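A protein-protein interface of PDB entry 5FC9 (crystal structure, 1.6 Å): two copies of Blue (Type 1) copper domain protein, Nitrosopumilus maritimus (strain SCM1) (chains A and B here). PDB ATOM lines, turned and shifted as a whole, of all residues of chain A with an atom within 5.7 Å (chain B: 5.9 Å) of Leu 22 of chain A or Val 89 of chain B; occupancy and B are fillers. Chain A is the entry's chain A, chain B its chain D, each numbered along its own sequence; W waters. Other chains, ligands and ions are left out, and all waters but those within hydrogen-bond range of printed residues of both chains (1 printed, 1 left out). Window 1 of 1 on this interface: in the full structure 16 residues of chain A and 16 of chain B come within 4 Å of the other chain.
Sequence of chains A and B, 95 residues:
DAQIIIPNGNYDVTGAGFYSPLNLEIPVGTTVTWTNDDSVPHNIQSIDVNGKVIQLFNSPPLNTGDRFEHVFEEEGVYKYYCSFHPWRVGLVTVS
The backbone NH (N) of Gly 15 of chain A lies close to the backbone carbonyl oxygen (O) of Pro 86 of chain B, 3.2 Å away.
Printed residues of chain B within 4 Å of Phe 18 of chain A: Lys 79.
Leu 22 of chain A touches three residues of chain B.
Leu 24 of chain A touches none of the printed residues of chain B.
Of the printed residues of chain A, Lys 79 of chain B touches Phe 18 (3.6 Å) and Leu 22 (3.2 Å).
Printed residues of chain A within 4 Å of Trp 87 of chain B: Thr 14 (3.5 Å) and Gly 15 (3.8 Å).
Of chain A, only Gly 15 and Leu 22 come within 4 Å of Val 89 of chain B.
Hydrophobic or aromatic side chains of chain A within 4 Å of the printed part of chain B: Phe 18, Leu 22, Val 89 and Leu 91.
Printed residues of chain B that touch a printed residue of chain A: Leu 22, Lys 79, Pro 86, Trp 87, Val 89 and Leu 91.
Hydrophobic or aromatic side chains of chain B that line the printed part of chain A: Leu 22, Pro 86, Trp 87, Val 89 and Leu 91.
Among the printed residues, 11 pairs touch across the chains.
Thr 14 of chain A touches Pro 86 of chain B (OG1 to CB, 3.7 Å).
CA of Trp 87 of chain B touches C of Thr 14 of chain A, at 3.5 Å.
Gly 15 of chain A touches Trp 87 of chain B (N to N, 3.8 Å).
CA of Gly 15 of chain A touches CG1 of Val 89 of chain B (3.96 Å).
Lys 79 of chain B touches Phe 18 of chain A.
Lys 79 of chain B touches Leu 22 of chain A (NZ to CB, 3.2 Å).
Leu 22 of chain A touches Val 89 of chain B.
CD2 of Leu 22 of chain A touches CD1 of Leu 91 of chain B, 3.9 Å away.
Leu 22 of chain B touches Val 89 of chain A (CD2 to CG2, 3.9 Å).
Leu 22 of chain B touches Leu 91 of chain A.
The backbone NH (N) of Ile 47 of chain B lies within hydrogen-bond range of the backbone carbonyl oxygen (O) of Lys 79 of chain B, at 3.0 Å.
The backbone carbonyl oxygen (O) of Leu 91 of chain A lies within hydrogen-bond range of the backbone NH (N) of Leu 24 of chain A (3.0 Å).
The backbone carbonyl oxygen (O) of Leu 22 of chain B sits at hydrogen-bond distance from the backbone NH (N) of Leu 91 of chain B, at 2.9 Å.
The backbone NH (N) of Leu 91 of chain A lies within hydrogen-bond range of the backbone carbonyl oxygen (O) of Leu 22 of chain A (2.9 Å).
Leu 22 of chain A touches Val 89 of chain B, and with the chains exchanged Val 89 of chain A touches Leu 22 of chain B.
Leu 22 of chain A touches Leu 91 of chain B, and with the chains exchanged Leu 91 of chain A touches Leu 22 of chain B.
Of the 11 pairs that touch across the chains among the printed residues, 4 have their exchanged pair printed and touching as well.
Water W1 lies within hydrogen-bond range of O of Tyr 19 of chain A (3.0 Å), N of Leu 22 of chain A (3.1 Å) and NZ of Lys 79 of chain B (3.5 Å).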
ATOM      1  N   THR A  14       6.904 -11.376  -7.230  1.00  0.00           N
ATOM      2  CA  THR A  14       5.766 -10.479  -7.111  1.00  0.00           C
ATOM      3  C   THR A  14       5.272 -10.517  -5.679  1.00  0.00           C
ATOM      4  O   THR A  14       5.888 -11.175  -4.830  1.00  0.00           O
ATOM      5  CB  THR A  14       4.634 -10.860  -8.100  1.00  0.00           C
ATOM      6  OG1 THR A  14       3.648  -9.823  -8.133  1.00  0.00           O
ATOM      7  CG2 THR A  14       3.974 -12.174  -7.687  1.00  0.00           C
ATOM      8  N   GLY A  15       4.182  -9.815  -5.392  1.00  0.00           N
ATOM      9  CA  GLY A  15       3.698  -9.755  -4.015  1.00  0.00           C
ATOM     10  C   GLY A  15       3.050 -11.042  -3.541  1.00  0.00           C
ATOM     11  O   GLY A  15       3.515 -11.680  -2.597  1.00  0.00           O
ATOM     12  N   ALA A  16       1.955 -11.421  -4.189  1.00  0.00           N
ATOM     13  CA  ALA A  16       1.251 -12.633  -3.789  1.00  0.00           C
ATOM     14  C   ALA A  16       2.195 -13.838  -3.810  1.00  0.00           C
ATOM     15  O   ALA A  16       3.088 -13.932  -4.661  1.00  0.00           O
ATOM     16  CB  ALA A  16       0.068 -12.875  -4.685  1.00  0.00           C
ATOM     17  N   PHE A  18       3.713 -14.742  -0.777  1.00  0.00           N
ATOM     18  CA  PHE A  18       4.614 -14.555   0.354  1.00  0.00           C
ATOM     19  C   PHE A  18       4.316 -15.563   1.471  1.00  0.00           C
ATOM     20  O   PHE A  18       3.278 -16.233   1.465  1.00  0.00           O
ATOM     21  CB  PHE A  18       4.551 -13.111   0.887  1.00  0.00           C
ATOM     22  CG  PHE A  18       3.156 -12.538   0.996  1.00  0.00           C
ATOM     23  CD1 PHE A  18       2.213 -13.116   1.826  1.00  0.00           C
ATOM     24  CD2 PHE A  18       2.816 -11.377   0.309  1.00  0.00           C
ATOM     25  CE1 PHE A  18       0.938 -12.582   1.930  1.00  0.00           C
ATOM     26  CE2 PHE A  18       1.552 -10.835   0.423  1.00  0.00           C
ATOM     27  CZ  PHE A  18       0.612 -11.438   1.228  1.00  0.00           C
ATOM     28  N   TYR A  19       5.255 -15.667   2.408  1.00  0.00           N
ATOM     29  CA  TYR A  19       5.123 -16.550   3.569  1.00  0.00           C
ATOM     30  C   TYR A  19       3.828 -16.289   4.312  1.00  0.00           C
ATOM     31  O   TYR A  19       3.396 -15.151   4.424  1.00  0.00           O
ATOM     32  CB  TYR A  19       6.298 -16.354   4.535  1.00  0.00           C
ATOM     33  CG  TYR A  19       7.661 -16.476   3.893  1.00  0.00           C
ATOM     34  CD1 TYR A  19       7.967 -17.544   3.055  1.00  0.00           C
ATOM     35  CD2 TYR A  19       8.633 -15.518   4.118  1.00  0.00           C
ATOM     36  CE1 TYR A  19       9.212 -17.653   2.456  1.00  0.00           C
ATOM     37  CE2 TYR A  19       9.880 -15.606   3.523  1.00  0.00           C
ATOM     38  CZ  TYR A  19      10.168 -16.678   2.692  1.00  0.00           C
ATOM     39  OH  TYR A  19      11.396 -16.797   2.083  1.00  0.00           O
ATOM     40  N   SER A  20       3.225 -17.355   4.839  1.00  0.00           N
ATOM     41  CA  SER A  20       1.939 -17.260   5.512  1.00  0.00           C
ATOM     42  C   SER A  20       2.009 -17.849   6.914  1.00  0.00           C
ATOM     43  O   SER A  20       2.114 -19.059   7.058  1.00  0.00           O
ATOM     44  CB  SER A  20       0.869 -17.991   4.698  1.00  0.00           C
ATOM     45  OG  SER A  20      -0.416 -17.820   5.263  1.00  0.00           O
ATOM     46  N   PRO A  21       1.933 -17.001   7.949  1.00  0.00           N
ATOM     47  CA  PRO A  21       1.790 -15.547   7.903  1.00  0.00           C
ATOM     48  C   PRO A  21       3.121 -14.863   7.655  1.00  0.00           C
ATOM     49  O   PRO A  21       4.170 -15.437   7.948  1.00  0.00           O
ATOM     50  CB  PRO A  21       1.275 -15.208   9.301  1.00  0.00           C
ATOM     51  CG  PRO A  21       1.866 -16.269  10.158  1.00  0.00           C
ATOM     52  CD  PRO A  21       1.831 -17.540   9.336  1.00  0.00           C
ATOM     53  N   LEU A  22       3.076 -13.637   7.151  1.00  0.00           N
ATOM     54  CA  LEU A  22       4.288 -12.903   6.835  1.00  0.00           C
ATOM     55  C   LEU A  22       4.985 -12.412   8.110  1.00  0.00           C
ATOM     56  O   LEU A  22       6.203 -12.249   8.136  1.00  0.00           O
ATOM     57  CB  LEU A  22       3.950 -11.738   5.911  1.00  0.00           C
ATOM     58  CG  LEU A  22       5.112 -11.030   5.226  1.00  0.00           C
ATOM     59  CD1 LEU A  22       5.953 -12.021   4.453  1.00  0.00           C
ATOM     60  CD2 LEU A  22       4.537  -9.963   4.309  1.00  0.00           C
ATOM     61  N   ASN A  23       4.197 -12.163   9.153  1.00  0.00           N
ATOM     62  CA  ASN A  23       4.731 -11.905  10.486  1.00  0.00           C
ATOM     63  C   ASN A  23       4.063 -12.863  11.450  1.00  0.00           C
ATOM     64  O   ASN A  23       2.860 -12.769  11.675  1.00  0.00           O
ATOM     65  CB  ASN A  23       4.494 -10.461  10.944  1.00  0.00           C
ATOM     66  CG  ASN A  23       5.042 -10.202  12.349  1.00  0.00           C
ATOM     67  OD1 ASN A  23       6.086 -10.735  12.720  1.00  0.00           O
ATOM     68  ND2 ASN A  23       4.331  -9.392  13.130  1.00  0.00           N
ATOM     69  N   LEU A  24       4.839 -13.797  11.986  1.00  0.00           N
ATOM     70  CA  LEU A  24       4.317 -14.757  12.950  1.00  0.00           C
ATOM     71  C   LEU A  24       4.550 -14.221  14.352  1.00  0.00           C
ATOM     72  O   LEU A  24       5.695 -14.027  14.746  1.00  0.00           O
ATOM     73  CB  LEU A  24       4.994 -16.119  12.776  1.00  0.00           C
ATOM     74  CG  LEU A  24       4.562 -17.178  13.796  1.00  0.00           C
ATOM     75  CD1 LEU A  24       3.154 -17.644  13.500  1.00  0.00           C
ATOM     76  CD2 LEU A  24       5.543 -18.356  13.842  1.00  0.00           C
ATOM     77  N   TYR A  80      13.887 -12.891   8.333  1.00  0.00           N
ATOM     78  CA  TYR A  80      14.527 -13.994   7.637  1.00  0.00           C
ATOM     79  C   TYR A  80      14.182 -13.947   6.164  1.00  0.00           C
ATOM     80  O   TYR A  80      13.210 -13.299   5.775  1.00  0.00           O
ATOM     81  CB  TYR A  80      14.106 -15.348   8.226  1.00  0.00           C
ATOM     82  CG  TYR A  80      12.644 -15.641   8.026  1.00  0.00           C
ATOM     83  CD1 TYR A  80      11.704 -15.212   8.942  1.00  0.00           C
ATOM     84  CD2 TYR A  80      12.205 -16.339   6.903  1.00  0.00           C
ATOM     85  CE1 TYR A  80      10.342 -15.466   8.761  1.00  0.00           C
ATOM     86  CE2 TYR A  80      10.853 -16.592   6.705  1.00  0.00           C
ATOM     87  CZ  TYR A  80       9.931 -16.157   7.629  1.00  0.00           C
ATOM     88  OH  TYR A  80       8.590 -16.405   7.449  1.00  0.00           O
ATOM     89  N   VAL A  89      10.993 -12.045   2.104  1.00  0.00           N
ATOM     90  CA  VAL A  89      11.463 -11.770   3.459  1.00  0.00           C
ATOM     91  C   VAL A  89      10.288 -11.749   4.432  1.00  0.00           C
ATOM     92  O   VAL A  89       9.253 -11.122   4.166  1.00  0.00           O
ATOM     93  CB  VAL A  89      12.236 -10.436   3.520  1.00  0.00           C
ATOM     94  CG1 VAL A  89      13.470 -10.504   2.642  1.00  0.00           C
ATOM     95  CG2 VAL A  89      11.359  -9.260   3.086  1.00  0.00           C
ATOM     96  N   GLY A  90      10.434 -12.467   5.548  1.00  0.00           N
ATOM     97  CA  GLY A  90       9.382 -12.524   6.543  1.00  0.00           C
ATOM     98  C   GLY A  90       9.893 -12.187   7.933  1.00  0.00           C
ATOM     99  O   GLY A  90      11.079 -11.903   8.113  1.00  0.00           O
ATOM    100  N   LEU A  91       8.982 -12.214   8.895  1.00  0.00           N
ATOM    101  CA  LEU A  91       9.281 -11.881  10.282  1.00  0.00           C
ATOM    102  C   LEU A  91       8.757 -12.922  11.247  1.00  0.00           C
ATOM    103  O   LEU A  91       7.701 -13.515  11.036  1.00  0.00           O
ATOM    104  CB  LEU A  91       8.668 -10.532  10.661  1.00  0.00           C
ATOM    105  CG  LEU A  91       9.029  -9.327   9.809  1.00  0.00           C
ATOM    106  CD1 LEU A  91       8.200  -8.161  10.268  1.00  0.00           C
ATOM    107  CD2 LEU A  91      10.479  -9.022  10.016  1.00  0.00           C
ATOM    108  N   VAL A  92       9.495 -13.107  12.338  1.00  0.00           N
ATOM    109  CA  VAL A  92       8.977 -13.760  13.530  1.00  0.00           C
ATOM    110  C   VAL A  92       9.090 -12.752  14.667  1.00  0.00           C
ATOM    111  O   VAL A  92      10.181 -12.256  14.952  1.00  0.00           O
ATOM    112  CB  VAL A  92       9.751 -15.041  13.881  1.00  0.00           C
ATOM    113  CG1 VAL A  92       9.201 -15.675  15.161  1.00  0.00           C
ATOM    114  CG2 VAL A  92       9.711 -16.033  12.733  1.00  0.00           C
ATOM    115  N   TYR B  19      11.287  -2.346   3.223  1.00  0.00           N
ATOM    116  CA  TYR B  19      10.741  -1.233   4.004  1.00  0.00           C
ATOM    117  C   TYR B  19      11.247  -1.294   5.438  1.00  0.00           C
ATOM    118  O   TYR B  19      11.376  -2.375   6.017  1.00  0.00           O
ATOM    119  CB  TYR B  19       9.216  -1.258   4.012  1.00  0.00           C
ATOM    120  CG  TYR B  19       8.581  -1.296   2.648  1.00  0.00           C
ATOM    121  CD1 TYR B  19       8.936  -0.373   1.671  1.00  0.00           C
ATOM    122  CD2 TYR B  19       7.616  -2.243   2.337  1.00  0.00           C
ATOM    123  CE1 TYR B  19       8.363  -0.397   0.422  1.00  0.00           C
ATOM    124  CE2 TYR B  19       7.030  -2.283   1.077  1.00  0.00           C
ATOM    125  CZ  TYR B  19       7.404  -1.347   0.124  1.00  0.00           C
ATOM    126  OH  TYR B  19       6.837  -1.375  -1.125  1.00  0.00           O
ATOM    127  N   LEU B  22       9.931  -3.329   8.559  1.00  0.00           N
ATOM    128  CA  LEU B  22       9.122  -4.191   7.706  1.00  0.00           C
ATOM    129  C   LEU B  22       7.720  -4.343   8.269  1.00  0.00           C
ATOM    130  O   LEU B  22       6.741  -4.434   7.527  1.00  0.00           O
ATOM    131  CB  LEU B  22       9.801  -5.555   7.553  1.00  0.00           C
ATOM    132  CG  LEU B  22       9.271  -6.482   6.463  1.00  0.00           C
ATOM    133  CD1 LEU B  22       9.353  -5.761   5.133  1.00  0.00           C
ATOM    134  CD2 LEU B  22      10.076  -7.779   6.430  1.00  0.00           C
ATOM    135  N   ILE B  47      -2.883  -3.912   0.445  1.00  0.00           N
ATOM    136  CA  ILE B  47      -3.257  -5.190  -0.171  1.00  0.00           C
ATOM    137  C   ILE B  47      -3.921  -6.083   0.871  1.00  0.00           C
ATOM    138  O   ILE B  47      -3.748  -5.858   2.066  1.00  0.00           O
ATOM    139  CB  ILE B  47      -2.039  -5.904  -0.797  1.00  0.00           C
ATOM    140  CG1 ILE B  47      -1.058  -6.368   0.287  1.00  0.00           C
ATOM    141  CG2 ILE B  47      -1.361  -4.976  -1.799  1.00  0.00           C
ATOM    142  CD1 ILE B  47       0.270  -6.872  -0.278  1.00  0.00           C
ATOM    143  N   LYS B  79      -1.381  -5.257   5.344  1.00  0.00           N
ATOM    144  CA  LYS B  79      -0.265  -5.394   4.415  1.00  0.00           C
ATOM    145  C   LYS B  79      -0.354  -4.321   3.335  1.00  0.00           C
ATOM    146  O   LYS B  79      -1.413  -3.742   3.082  1.00  0.00           O
ATOM    147  CB  LYS B  79      -0.243  -6.791   3.782  1.00  0.00           C
ATOM    148  CG  LYS B  79      -0.006  -7.930   4.770  1.00  0.00           C
ATOM    149  CD  LYS B  79       0.120  -9.267   4.036  1.00  0.00           C
ATOM    150  CE  LYS B  79      -0.103 -10.456   4.981  1.00  0.00           C
ATOM    151  NZ  LYS B  79       0.953 -10.494   6.018  1.00  0.00           N
ATOM    152  N   TYR B  80       0.777  -4.047   2.705  1.00  0.00           N
ATOM    153  CA  TYR B  80       0.797  -3.101   1.604  1.00  0.00           C
ATOM    154  C   TYR B  80       1.959  -3.453   0.699  1.00  0.00           C
ATOM    155  O   TYR B  80       2.894  -4.144   1.109  1.00  0.00           O
ATOM    156  CB  TYR B  80       0.909  -1.649   2.108  1.00  0.00           C
ATOM    157  CG  TYR B  80       2.213  -1.374   2.834  1.00  0.00           C
ATOM    158  CD1 TYR B  80       2.328  -1.571   4.206  1.00  0.00           C
ATOM    159  CD2 TYR B  80       3.331  -0.921   2.140  1.00  0.00           C
ATOM    160  CE1 TYR B  80       3.538  -1.339   4.872  1.00  0.00           C
ATOM    161  CE2 TYR B  80       4.528  -0.684   2.788  1.00  0.00           C
ATOM    162  CZ  TYR B  80       4.632  -0.896   4.151  1.00  0.00           C
ATOM    163  OH  TYR B  80       5.827  -0.649   4.785  1.00  0.00           O
ATOM    164  N   TYR B  81       1.861  -3.031  -0.555  1.00  0.00           N
ATOM    165  CA  TYR B  81       3.014  -3.099  -1.437  1.00  0.00           C
ATOM    166  C   TYR B  81       3.144  -1.826  -2.257  1.00  0.00           C
ATOM    167  O   TYR B  81       2.572  -0.794  -1.927  1.00  0.00           O
ATOM    168  CB  TYR B  81       2.999  -4.352  -2.350  1.00  0.00           C
ATOM    169  CG  TYR B  81       1.941  -4.543  -3.428  1.00  0.00           C
ATOM    170  CD1 TYR B  81       1.322  -3.474  -4.078  1.00  0.00           C
ATOM    171  CD2 TYR B  81       1.709  -5.824  -3.933  1.00  0.00           C
ATOM    172  CE1 TYR B  81       0.412  -3.696  -5.116  1.00  0.00           C
ATOM    173  CE2 TYR B  81       0.817  -6.045  -4.977  1.00  0.00           C
ATOM    174  CZ  TYR B  81       0.162  -4.970  -5.553  1.00  0.00           C
ATOM    175  OH  TYR B  81      -0.726  -5.147  -6.594  1.00  0.00           O
ATOM    176  N   CYS B  82       3.960  -1.909  -3.297  1.00  0.00           N
ATOM    177  CA  CYS B  82       4.163  -0.815  -4.229  1.00  0.00           C
ATOM    178  C   CYS B  82       3.758  -1.301  -5.609  1.00  0.00           C
ATOM    179  O   CYS B  82       4.189  -2.373  -6.038  1.00  0.00           O
ATOM    180  CB  CYS B  82       5.622  -0.384  -4.193  1.00  0.00           C
ATOM    181  SG  CYS B  82       6.111   0.769  -5.495  1.00  0.00           S
ATOM    182  N   HIS B  85       6.723  -1.997  -7.744  1.00  0.00           N
ATOM    183  CA  HIS B  85       7.564  -3.113  -7.282  1.00  0.00           C
ATOM    184  C   HIS B  85       6.766  -4.032  -6.359  1.00  0.00           C
ATOM    185  O   HIS B  85       6.939  -3.995  -5.132  1.00  0.00           O
ATOM    186  CB  HIS B  85       8.801  -2.592  -6.548  1.00  0.00           C
ATOM    187  CG  HIS B  85       9.498  -1.479  -7.267  1.00  0.00           C
ATOM    188  ND1 HIS B  85       9.399  -0.160  -6.877  1.00  0.00           N
ATOM    189  CD2 HIS B  85      10.278  -1.490  -8.373  1.00  0.00           C
ATOM    190  CE1 HIS B  85      10.094   0.594  -7.710  1.00  0.00           C
ATOM    191  NE2 HIS B  85      10.645  -0.187  -8.623  1.00  0.00           N
ATOM    192  N   PRO B  86       5.874  -4.849  -6.936  1.00  0.00           N
ATOM    193  CA  PRO B  86       4.912  -5.592  -6.117  1.00  0.00           C
ATOM    194  C   PRO B  86       5.537  -6.581  -5.139  1.00  0.00           C
ATOM    195  O   PRO B  86       4.885  -6.899  -4.142  1.00  0.00           O
ATOM    196  CB  PRO B  86       4.067  -6.329  -7.161  1.00  0.00           C
ATOM    197  CG  PRO B  86       4.127  -5.448  -8.362  1.00  0.00           C
ATOM    198  CD  PRO B  86       5.542  -4.916  -8.371  1.00  0.00           C
ATOM    199  N   TRP B  87       6.767  -7.027  -5.387  1.00  0.00           N
ATOM    200  CA  TRP B  87       7.416  -7.965  -4.468  1.00  0.00           C
ATOM    201  C   TRP B  87       7.812  -7.295  -3.154  1.00  0.00           C
ATOM    202  O   TRP B  87       8.105  -7.978  -2.166  1.00  0.00           O
ATOM    203  CB  TRP B  87       8.653  -8.601  -5.114  1.00  0.00           C
ATOM    204  CG  TRP B  87       9.741  -7.607  -5.397  1.00  0.00           C
ATOM    205  CD1 TRP B  87      10.780  -7.258  -4.578  1.00  0.00           C
ATOM    206  CD2 TRP B  87       9.876  -6.821  -6.576  1.00  0.00           C
ATOM    207  NE1 TRP B  87      11.561  -6.302  -5.189  1.00  0.00           N
ATOM    208  CE2 TRP B  87      11.026  -6.022  -6.421  1.00  0.00           C
ATOM    209  CE3 TRP B  87       9.144  -6.733  -7.766  1.00  0.00           C
ATOM    210  CZ2 TRP B  87      11.450  -5.128  -7.402  1.00  0.00           C
ATOM    211  CZ3 TRP B  87       9.560  -5.851  -8.728  1.00  0.00           C
ATOM    212  CH2 TRP B  87      10.705  -5.058  -8.545  1.00  0.00           C
ATOM    213  N   ARG B  88       7.832  -5.963  -3.133  1.00  0.00           N
ATOM    214  CA  ARG B  88       8.156  -5.254  -1.899  1.00  0.00           C
ATOM    215  C   ARG B  88       6.898  -5.075  -1.062  1.00  0.00           C
ATOM    216  O   ARG B  88       6.081  -4.179  -1.319  1.00  0.00           O
ATOM    217  CB  ARG B  88       8.802  -3.905  -2.206  1.00  0.00           C
ATOM    218  CG  ARG B  88      10.172  -4.010  -2.867  1.00  0.00           C
ATOM    219  CD  ARG B  88      11.178  -4.771  -2.013  1.00  0.00           C
ATOM    220  NE  ARG B  88      12.537  -4.450  -2.443  1.00  0.00           N
ATOM    221  CZ  ARG B  88      13.647  -4.963  -1.921  1.00  0.00           C
ATOM    222  NH1 ARG B  88      13.581  -5.876  -0.965  1.00  0.00           N
ATOM    223  NH2 ARG B  88      14.832  -4.576  -2.381  1.00  0.00           N
ATOM    224  N   VAL B  89       6.759  -5.947  -0.068  1.00  0.00           N
ATOM    225  CA  VAL B  89       5.576  -6.029   0.785  1.00  0.00           C
ATOM    226  C   VAL B  89       5.933  -5.699   2.229  1.00  0.00           C
ATOM    227  O   VAL B  89       6.900  -6.238   2.769  1.00  0.00           O
ATOM    228  CB  VAL B  89       4.933  -7.445   0.709  1.00  0.00           C
ATOM    229  CG1 VAL B  89       4.477  -7.735  -0.704  1.00  0.00           C
ATOM    230  CG2 VAL B  89       5.900  -8.524   1.153  1.00  0.00           C
ATOM    231  N   GLY B  90       5.152  -4.819   2.848  1.00  0.00           N
ATOM    232  CA  GLY B  90       5.340  -4.495   4.251  1.00  0.00           C
ATOM    233  C   GLY B  90       4.051  -4.654   5.035  1.00  0.00           C
ATOM    234  O   GLY B  90       2.990  -4.963   4.469  1.00  0.00           O
ATOM    235  N   LEU B  91       4.131  -4.437   6.346  1.00  0.00           N
ATOM    236  CA  LEU B  91       2.955  -4.513   7.206  1.00  0.00           C
ATOM    237  C   LEU B  91       2.876  -3.349   8.169  1.00  0.00           C
ATOM    238  O   LEU B  91       3.890  -2.810   8.599  1.00  0.00           O
ATOM    239  CB  LEU B  91       2.937  -5.801   8.031  1.00  0.00           C
ATOM    240  CG  LEU B  91       3.175  -7.138   7.344  1.00  0.00           C
ATOM    241  CD1 LEU B  91       4.667  -7.438   7.273  1.00  0.00           C
ATOM    242  CD2 LEU B  91       2.454  -8.222   8.119  1.00  0.00           C
HETATM  243  O   HOH W   1       0.818 -13.832   5.081  1.00  0.00           O
